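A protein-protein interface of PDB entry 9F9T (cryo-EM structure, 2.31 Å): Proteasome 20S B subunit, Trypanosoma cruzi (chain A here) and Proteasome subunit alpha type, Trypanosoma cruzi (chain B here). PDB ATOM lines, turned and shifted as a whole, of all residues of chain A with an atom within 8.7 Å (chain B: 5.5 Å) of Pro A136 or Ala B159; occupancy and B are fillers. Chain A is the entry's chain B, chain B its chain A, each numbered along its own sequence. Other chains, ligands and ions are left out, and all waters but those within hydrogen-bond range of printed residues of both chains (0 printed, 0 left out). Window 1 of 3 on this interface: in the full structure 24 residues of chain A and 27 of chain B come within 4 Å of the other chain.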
ATOM      1  N   LYS A 119      19.070  36.507   3.842  1.00  0.00           N
ATOM      2  CA  LYS A 119      18.114  37.389   4.479  1.00  0.00           C
ATOM      3  C   LYS A 119      17.268  38.120   3.460  1.00  0.00           C
ATOM      4  O   LYS A 119      16.085  38.371   3.658  1.00  0.00           O
ATOM      5  CB  LYS A 119      18.916  38.335   5.336  1.00  0.00           C
ATOM      6  CG  LYS A 119      19.236  37.710   6.692  1.00  0.00           C
ATOM      7  CD  LYS A 119      18.101  37.937   7.697  1.00  0.00           C
ATOM      8  CE  LYS A 119      18.435  37.571   9.131  1.00  0.00           C
ATOM      9  NZ  LYS A 119      18.870  36.155   9.238  1.00  0.00           N
ATOM     10  N   PHE A 121      15.633  37.768  -0.420  1.00  0.00           N
ATOM     11  CA  PHE A 121      15.215  36.694  -1.316  1.00  0.00           C
ATOM     12  C   PHE A 121      14.631  37.214  -2.618  1.00  0.00           C
ATOM     13  O   PHE A 121      13.922  38.196  -2.667  1.00  0.00           O
ATOM     14  CB  PHE A 121      14.137  35.809  -0.708  1.00  0.00           C
ATOM     15  CG  PHE A 121      14.594  35.160   0.556  1.00  0.00           C
ATOM     16  CD1 PHE A 121      15.280  33.990   0.525  1.00  0.00           C
ATOM     17  CD2 PHE A 121      14.471  35.790   1.777  1.00  0.00           C
ATOM     18  CE1 PHE A 121      15.718  33.385   1.689  1.00  0.00           C
ATOM     19  CE2 PHE A 121      14.937  35.207   2.946  1.00  0.00           C
ATOM     20  CZ  PHE A 121      15.593  34.023   2.892  1.00  0.00           C
ATOM     21  N   TYR A 131      12.879  39.967   5.757  1.00  0.00           N
ATOM     22  CA  TYR A 131      12.006  39.676   6.862  1.00  0.00           C
ATOM     23  C   TYR A 131      12.773  39.966   8.131  1.00  0.00           C
ATOM     24  O   TYR A 131      13.999  40.073   8.166  1.00  0.00           O
ATOM     25  CB  TYR A 131      11.611  38.202   6.792  1.00  0.00           C
ATOM     26  CG  TYR A 131      12.681  37.247   7.316  1.00  0.00           C
ATOM     27  CD1 TYR A 131      12.805  36.890   8.649  1.00  0.00           C
ATOM     28  CD2 TYR A 131      13.698  36.822   6.486  1.00  0.00           C
ATOM     29  CE1 TYR A 131      13.907  36.168   9.147  1.00  0.00           C
ATOM     30  CE2 TYR A 131      14.725  35.990   6.928  1.00  0.00           C
ATOM     31  CZ  TYR A 131      14.847  35.667   8.268  1.00  0.00           C
ATOM     32  OH  TYR A 131      15.896  34.831   8.561  1.00  0.00           O
ATOM     33  N   GLY A 133      12.239  38.290  12.313  1.00  0.00           N
ATOM     34  CA  GLY A 133      11.528  37.451  13.255  1.00  0.00           C
ATOM     35  C   GLY A 133      11.987  36.022  13.057  1.00  0.00           C
ATOM     36  O   GLY A 133      13.186  35.818  13.006  1.00  0.00           O
ATOM     37  N   ILE A 134      11.057  35.093  12.822  1.00  0.00           N
ATOM     38  CA  ILE A 134      11.395  33.684  12.783  1.00  0.00           C
ATOM     39  C   ILE A 134      11.706  33.217  11.364  1.00  0.00           C
ATOM     40  O   ILE A 134      10.817  32.967  10.544  1.00  0.00           O
ATOM     41  CB  ILE A 134      10.249  32.895  13.431  1.00  0.00           C
ATOM     42  CG1 ILE A 134      10.100  33.259  14.913  1.00  0.00           C
ATOM     43  CG2 ILE A 134      10.410  31.372  13.274  1.00  0.00           C
ATOM     44  CD1 ILE A 134       8.924  32.505  15.500  1.00  0.00           C
ATOM     45  N   GLY A 135      12.991  32.964  11.131  1.00  0.00           N
ATOM     46  CA  GLY A 135      13.457  32.596   9.809  1.00  0.00           C
ATOM     47  C   GLY A 135      12.602  31.519   9.148  1.00  0.00           C
ATOM     48  O   GLY A 135      12.104  31.693   8.030  1.00  0.00           O
ATOM     49  N   PRO A 136      12.471  30.363   9.821  1.00  0.00           N
ATOM     50  CA  PRO A 136      11.793  29.210   9.255  1.00  0.00           C
ATOM     51  C   PRO A 136      10.362  29.537   8.831  1.00  0.00           C
ATOM     52  O   PRO A 136       9.948  29.162   7.709  1.00  0.00           O
ATOM     53  CB  PRO A 136      11.868  28.169  10.394  1.00  0.00           C
ATOM     54  CG  PRO A 136      13.025  28.608  11.279  1.00  0.00           C
ATOM     55  CD  PRO A 136      13.099  30.109  11.133  1.00  0.00           C
ATOM     56  N   ASP A 137       9.654  30.393   9.606  1.00  0.00           N
ATOM     57  CA  ASP A 137       8.325  30.854   9.164  1.00  0.00           C
ATOM     58  C   ASP A 137       8.385  31.659   7.888  1.00  0.00           C
ATOM     59  O   ASP A 137       7.557  31.468   7.007  1.00  0.00           O
ATOM     60  CB  ASP A 137       7.577  31.682  10.214  1.00  0.00           C
ATOM     61  CG  ASP A 137       7.109  30.930  11.457  1.00  0.00           C
ATOM     62  OD1 ASP A 137       7.446  29.754  11.598  1.00  0.00           O
ATOM     63  OD2 ASP A 137       6.335  31.551  12.306  1.00  0.00           O
ATOM     64  N   CYS A 138       9.416  32.498   7.752  1.00  0.00           N
ATOM     65  CA  CYS A 138       9.630  33.234   6.510  1.00  0.00           C
ATOM     66  C   CYS A 138       9.780  32.333   5.269  1.00  0.00           C
ATOM     67  O   CYS A 138       9.272  32.712   4.179  1.00  0.00           O
ATOM     68  CB  CYS A 138      10.827  34.173   6.602  1.00  0.00           C
ATOM     69  SG  CYS A 138      10.899  35.334   5.193  1.00  0.00           S
ATOM     70  N   ARG A 139      10.479  31.166   5.393  1.00  0.00           N
ATOM     71  CA  ARG A 139      10.564  30.286   4.236  1.00  0.00           C
ATOM     72  C   ARG A 139       9.183  29.830   3.716  1.00  0.00           C
ATOM     73  O   ARG A 139       8.942  29.768   2.505  1.00  0.00           O
ATOM     74  CB  ARG A 139      11.377  29.028   4.454  1.00  0.00           C
ATOM     75  CG  ARG A 139      12.833  29.241   4.818  1.00  0.00           C
ATOM     76  CD  ARG A 139      13.533  27.933   4.371  1.00  0.00           C
ATOM     77  NE  ARG A 139      13.139  26.731   5.095  1.00  0.00           N
ATOM     78  CZ  ARG A 139      13.350  26.533   6.393  1.00  0.00           C
ATOM     79  NH1 ARG A 139      14.290  27.189   7.047  1.00  0.00           N
ATOM     80  NH2 ARG A 139      12.622  25.645   7.052  1.00  0.00           N
ATOM     81  N   VAL A 140       8.243  29.514   4.577  1.00  0.00           N
ATOM     82  CA  VAL A 140       6.912  29.172   4.110  1.00  0.00           C
ATOM     83  C   VAL A 140       6.340  30.276   3.218  1.00  0.00           C
ATOM     84  O   VAL A 140       5.711  29.980   2.219  1.00  0.00           O
ATOM     85  CB  VAL A 140       5.962  28.910   5.297  1.00  0.00           C
ATOM     86  CG1 VAL A 140       4.509  28.693   4.848  1.00  0.00           C
ATOM     87  CG2 VAL A 140       6.458  27.790   6.200  1.00  0.00           C
ATOM     88  N   LEU A 141       6.501  31.547   3.601  1.00  0.00           N
ATOM     89  CA  LEU A 141       5.867  32.626   2.855  1.00  0.00           C
ATOM     90  C   LEU A 141       6.594  32.889   1.530  1.00  0.00           C
ATOM     91  O   LEU A 141       5.963  33.142   0.481  1.00  0.00           O
ATOM     92  CB  LEU A 141       5.847  33.901   3.703  1.00  0.00           C
ATOM     93  CG  LEU A 141       5.079  33.797   5.025  1.00  0.00           C
ATOM     94  CD1 LEU A 141       5.579  34.781   6.072  1.00  0.00           C
ATOM     95  CD2 LEU A 141       3.599  33.935   4.821  1.00  0.00           C
ATOM     96  N   VAL A 142       7.929  32.825   1.591  1.00  0.00           N
ATOM     97  CA  VAL A 142       8.747  32.939   0.395  1.00  0.00           C
ATOM     98  C   VAL A 142       8.354  31.858  -0.616  1.00  0.00           C
ATOM     99  O   VAL A 142       8.056  32.176  -1.793  1.00  0.00           O
ATOM    100  CB  VAL A 142      10.220  32.893   0.775  1.00  0.00           C
ATOM    101  CG1 VAL A 142      11.110  32.726  -0.399  1.00  0.00           C
ATOM    102  CG2 VAL A 142      10.673  34.136   1.507  1.00  0.00           C
ATOM    103  N   ASP A 143       8.241  30.594  -0.154  1.00  0.00           N
ATOM    104  CA  ASP A 143       7.770  29.548  -1.062  1.00  0.00           C
ATOM    105  C   ASP A 143       6.395  29.841  -1.643  1.00  0.00           C
ATOM    106  O   ASP A 143       6.253  29.778  -2.866  1.00  0.00           O
ATOM    107  CB  ASP A 143       7.941  28.166  -0.457  1.00  0.00           C
ATOM    108  CG  ASP A 143       9.429  27.779  -0.270  1.00  0.00           C
ATOM    109  OD1 ASP A 143      10.370  28.311  -1.070  1.00  0.00           O
ATOM    110  OD2 ASP A 143       9.703  26.959   0.692  1.00  0.00           O
ATOM    111  N   ARG A 183      -0.673  28.088  14.832  1.00  0.00           N
ATOM    112  CA  ARG A 183      -0.288  29.382  15.304  1.00  0.00           C
ATOM    113  C   ARG A 183       0.009  30.336  14.159  1.00  0.00           C
ATOM    114  O   ARG A 183       0.209  29.940  13.022  1.00  0.00           O
ATOM    115  CB  ARG A 183       0.950  29.380  16.181  1.00  0.00           C
ATOM    116  CG  ARG A 183       2.212  28.911  15.495  1.00  0.00           C
ATOM    117  CD  ARG A 183       3.406  29.347  16.286  1.00  0.00           C
ATOM    118  NE  ARG A 183       4.554  28.747  15.621  1.00  0.00           N
ATOM    119  CZ  ARG A 183       5.097  29.208  14.511  1.00  0.00           C
ATOM    120  NH1 ARG A 183       6.106  28.572  13.965  1.00  0.00           N
ATOM    121  NH2 ARG A 183       4.673  30.339  13.959  1.00  0.00           N
ATOM    122  N   PHE A 185       2.209  33.096  11.893  1.00  0.00           N
ATOM    123  CA  PHE A 185       3.559  33.321  11.416  1.00  0.00           C
ATOM    124  C   PHE A 185       4.270  34.348  12.260  1.00  0.00           C
ATOM    125  O   PHE A 185       3.738  35.400  12.548  1.00  0.00           O
ATOM    126  CB  PHE A 185       3.522  33.888   9.998  1.00  0.00           C
ATOM    127  CG  PHE A 185       3.066  32.880   8.987  1.00  0.00           C
ATOM    128  CD1 PHE A 185       3.847  31.773   8.711  1.00  0.00           C
ATOM    129  CD2 PHE A 185       1.820  32.977   8.409  1.00  0.00           C
ATOM    130  CE1 PHE A 185       3.406  30.833   7.793  1.00  0.00           C
ATOM    131  CE2 PHE A 185       1.373  32.026   7.503  1.00  0.00           C
ATOM    132  CZ  PHE A 185       2.172  30.946   7.203  1.00  0.00           C
ATOM    133  N   GLY A 186       5.452  34.068  12.727  1.00  0.00           N
ATOM    134  CA  GLY A 186       6.031  35.049  13.626  1.00  0.00           C
ATOM    135  C   GLY A 186       7.082  35.921  12.959  1.00  0.00           C
ATOM    136  O   GLY A 186       8.180  36.054  13.465  1.00  0.00           O
ATOM    137  N   CYS A 187       6.727  36.488  11.810  1.00  0.00           N
ATOM    138  CA  CYS A 187       7.685  37.274  11.046  1.00  0.00           C
ATOM    139  C   CYS A 187       6.956  38.390  10.288  1.00  0.00           C
ATOM    140  O   CYS A 187       5.852  38.246   9.909  1.00  0.00           O
ATOM    141  CB  CYS A 187       8.472  36.369  10.087  1.00  0.00           C
ATOM    142  SG  CYS A 187       7.391  35.840   8.730  1.00  0.00           S
ATOM    143  N   VAL B  22       9.766  24.012  21.135  1.00  0.00           N
ATOM    144  CA  VAL B  22      11.014  24.164  20.436  1.00  0.00           C
ATOM    145  C   VAL B  22      12.142  24.252  21.442  1.00  0.00           C
ATOM    146  O   VAL B  22      13.060  23.440  21.370  1.00  0.00           O
ATOM    147  CB  VAL B  22      11.028  25.350  19.451  1.00  0.00           C
ATOM    148  CG1 VAL B  22      12.353  25.405  18.717  1.00  0.00           C
ATOM    149  CG2 VAL B  22       9.887  25.277  18.447  1.00  0.00           C
ATOM    150  N   PHE B  26      15.137  21.239  21.980  1.00  0.00           N
ATOM    151  CA  PHE B  26      16.574  21.469  22.026  1.00  0.00           C
ATOM    152  C   PHE B  26      17.187  20.852  23.251  1.00  0.00           C
ATOM    153  O   PHE B  26      18.312  20.447  23.164  1.00  0.00           O
ATOM    154  CB  PHE B  26      16.976  22.948  22.076  1.00  0.00           C
ATOM    155  CG  PHE B  26      17.229  23.552  20.726  1.00  0.00           C
ATOM    156  CD1 PHE B  26      18.446  23.347  20.086  1.00  0.00           C
ATOM    157  CD2 PHE B  26      16.218  24.173  20.037  1.00  0.00           C
ATOM    158  CE1 PHE B  26      18.679  23.847  18.809  1.00  0.00           C
ATOM    159  CE2 PHE B  26      16.444  24.710  18.774  1.00  0.00           C
ATOM    160  CZ  PHE B  26      17.682  24.546  18.158  1.00  0.00           C
ATOM    161  N   ALA B 119      10.520  20.012   9.787  1.00  0.00           N
ATOM    162  CA  ALA B 119      10.524  20.380  11.177  1.00  0.00           C
ATOM    163  C   ALA B 119       9.625  21.595  11.419  1.00  0.00           C
ATOM    164  O   ALA B 119       8.842  21.593  12.354  1.00  0.00           O
ATOM    165  CB  ALA B 119      11.927  20.640  11.638  1.00  0.00           C
ATOM    166  N   GLN B 120       9.740  22.629  10.572  1.00  0.00           N
ATOM    167  CA  GLN B 120       9.073  23.893  10.776  1.00  0.00           C
ATOM    168  C   GLN B 120       7.591  23.607  10.901  1.00  0.00           C
ATOM    169  O   GLN B 120       6.915  24.214  11.732  1.00  0.00           O
ATOM    170  CB  GLN B 120       9.358  24.826   9.587  1.00  0.00           C
ATOM    171  CG  GLN B 120       8.753  26.231   9.562  1.00  0.00           C
ATOM    172  CD  GLN B 120       7.274  26.291   9.329  1.00  0.00           C
ATOM    173  OE1 GLN B 120       6.676  25.612   8.481  1.00  0.00           O
ATOM    174  NE2 GLN B 120       6.652  27.119  10.123  1.00  0.00           N
ATOM    175  N   THR B 123       6.387  22.865  14.200  1.00  0.00           N
ATOM    176  CA  THR B 123       6.389  24.012  15.090  1.00  0.00           C
ATOM    177  C   THR B 123       5.147  24.892  14.950  1.00  0.00           C
ATOM    178  O   THR B 123       4.965  25.762  15.763  1.00  0.00           O
ATOM    179  CB  THR B 123       7.587  24.939  14.900  1.00  0.00           C
ATOM    180  OG1 THR B 123       7.463  25.556  13.633  1.00  0.00           O
ATOM    181  CG2 THR B 123       8.899  24.177  15.071  1.00  0.00           C
ATOM    182  N   ASP B 157      17.886  21.846  12.769  1.00  0.00           N
ATOM    183  CA  ASP B 157      17.538  21.656  14.159  1.00  0.00           C
ATOM    184  C   ASP B 157      16.039  21.647  14.328  1.00  0.00           C
ATOM    185  O   ASP B 157      15.287  21.698  13.336  1.00  0.00           O
ATOM    186  CB  ASP B 157      18.304  22.649  15.006  1.00  0.00           C
ATOM    187  CG  ASP B 157      17.906  24.062  14.708  1.00  0.00           C
ATOM    188  OD1 ASP B 157      18.771  24.970  14.913  1.00  0.00           O
ATOM    189  OD2 ASP B 157      16.733  24.241  14.339  1.00  0.00           O
ATOM    190  N   PRO B 158      15.566  21.442  15.561  1.00  0.00           N
ATOM    191  CA  PRO B 158      14.156  21.254  15.791  1.00  0.00           C
ATOM    192  C   PRO B 158      13.355  22.494  15.434  1.00  0.00           C
ATOM    193  O   PRO B 158      12.177  22.339  15.139  1.00  0.00           O
ATOM    194  CB  PRO B 158      14.043  20.987  17.290  1.00  0.00           C
ATOM    195  CG  PRO B 158      15.405  20.441  17.633  1.00  0.00           C
ATOM    196  CD  PRO B 158      16.347  21.254  16.776  1.00  0.00           C
ATOM    197  N   ALA B 159      13.958  23.686  15.437  1.00  0.00           N
ATOM    198  CA  ALA B 159      13.197  24.866  15.078  1.00  0.00           C
ATOM    199  C   ALA B 159      12.916  24.942  13.576  1.00  0.00           C
ATOM    200  O   ALA B 159      12.248  25.848  13.130  1.00  0.00           O
ATOM    201  CB  ALA B 159      13.926  26.118  15.487  1.00  0.00           C
ATOM    202  N   GLY B 160      13.539  24.071  12.793  1.00  0.00           N
ATOM    203  CA  GLY B 160      13.484  24.176  11.346  1.00  0.00           C
ATOM    204  C   GLY B 160      14.553  25.070  10.732  1.00  0.00           C
ATOM    205  O   GLY B 160      14.386  25.530   9.612  1.00  0.00           O
ATOM    206  N   TRP B 161      15.567  25.369  11.504  1.00  0.00           N
ATOM    207  CA  TRP B 161      16.661  26.148  11.018  1.00  0.00           C
ATOM    208  C   TRP B 161      17.671  25.252  10.286  1.00  0.00           C
ATOM    209  O   TRP B 161      18.025  24.191  10.744  1.00  0.00           O
ATOM    210  CB  TRP B 161      17.352  26.850  12.181  1.00  0.00           C
ATOM    211  CG  TRP B 161      18.409  27.807  11.729  1.00  0.00           C
ATOM    212  CD1 TRP B 161      18.252  29.067  11.219  1.00  0.00           C
ATOM    213  CD2 TRP B 161      19.823  27.520  11.715  1.00  0.00           C
ATOM    214  NE1 TRP B 161      19.479  29.593  10.901  1.00  0.00           N
ATOM    215  CE2 TRP B 161      20.461  28.673  11.198  1.00  0.00           C
ATOM    216  CE3 TRP B 161      20.603  26.408  12.087  1.00  0.00           C
ATOM    217  CZ2 TRP B 161      21.850  28.732  11.051  1.00  0.00           C
ATOM    218  CZ3 TRP B 161      21.974  26.475  11.947  1.00  0.00           C
ATOM    219  CH2 TRP B 161      22.584  27.623  11.430  1.00  0.00           C
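The backbone NH of Ala B159 is in hydrogen-bond range of the side-chain carboxylate of Asp B157, at 3.0 Å. NH2 of Arg A183 lies within salt-bridge range of OD2 of Asp A137 (2.6 Å). The side-chain carboxylate (OD2) of Asp A137 is in hydrogen-bond range of the backbone NH (N) of Gly A186 (2.7 Å).
Pro A136 touches Gln B120 (O to CG, 3.7 Å). Ala B159 touches Pro A136 (O to CG, 3.4 Å). Pro A136 touches Gly B160. Gln B120 touches Val A140.
The side-chain carboxylate (OD1) of Asp A137 sits at hydrogen-bond distance from the side-chain amide nitrogen (NE2) of Gln B120 (3.1 Å). The backbone carbonyl oxygen (O) of Thr B123 sits at hydrogen-bond distance from the guanidinium group (NE) of Arg A183 (3.0 Å). O of Gly B160 lies within hydrogen-bond range of NH1 of Arg A139, 3.1 Å away.
Of the 10 printed residues of chain B, 4 touch a printed residue of chain A. Printed residues of chain B that touch a printed residue of chain A: Gln B120, Thr B123, Ala B159 and Gly B160. Printed residues of chain A that touch a printed residue of chain B: Pro A136, Asp A137, Arg A139, Val A140 and Arg A183. Hydrophobic or aromatic side chains of chain A that line the printed part of chain B: Pro A136 and Val A140.
Of chain B, only Gln B120, Ala B159 and Gly B160 come within 4 Å of Pro A136. Of the printed residues of chain B, Asp A137 touches Gln B120. Printed residues of chain B within 4 Å of Arg A139: Gly B160 (3.1 Å). Of the printed residues of chain B, Val A140 touches Gln B120. Val A142 touches none of the printed residues of chain B. Of the printed residues of chain B, Arg A183 touches Thr B123. Of the printed residues of chain A, Thr B123 touches Arg A183. Gly B160 touches two residues of chain A. The nearest residue of chain B that does not touch Pro A136 is Trp B161 (4.1 Å). The nearest residue of chain A that does not touch Ala B159 is Ile A134 (5.8 Å). The nearest printed residue of chain B that does not touch Asp A137 is Thr B123 (4.7 Å).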
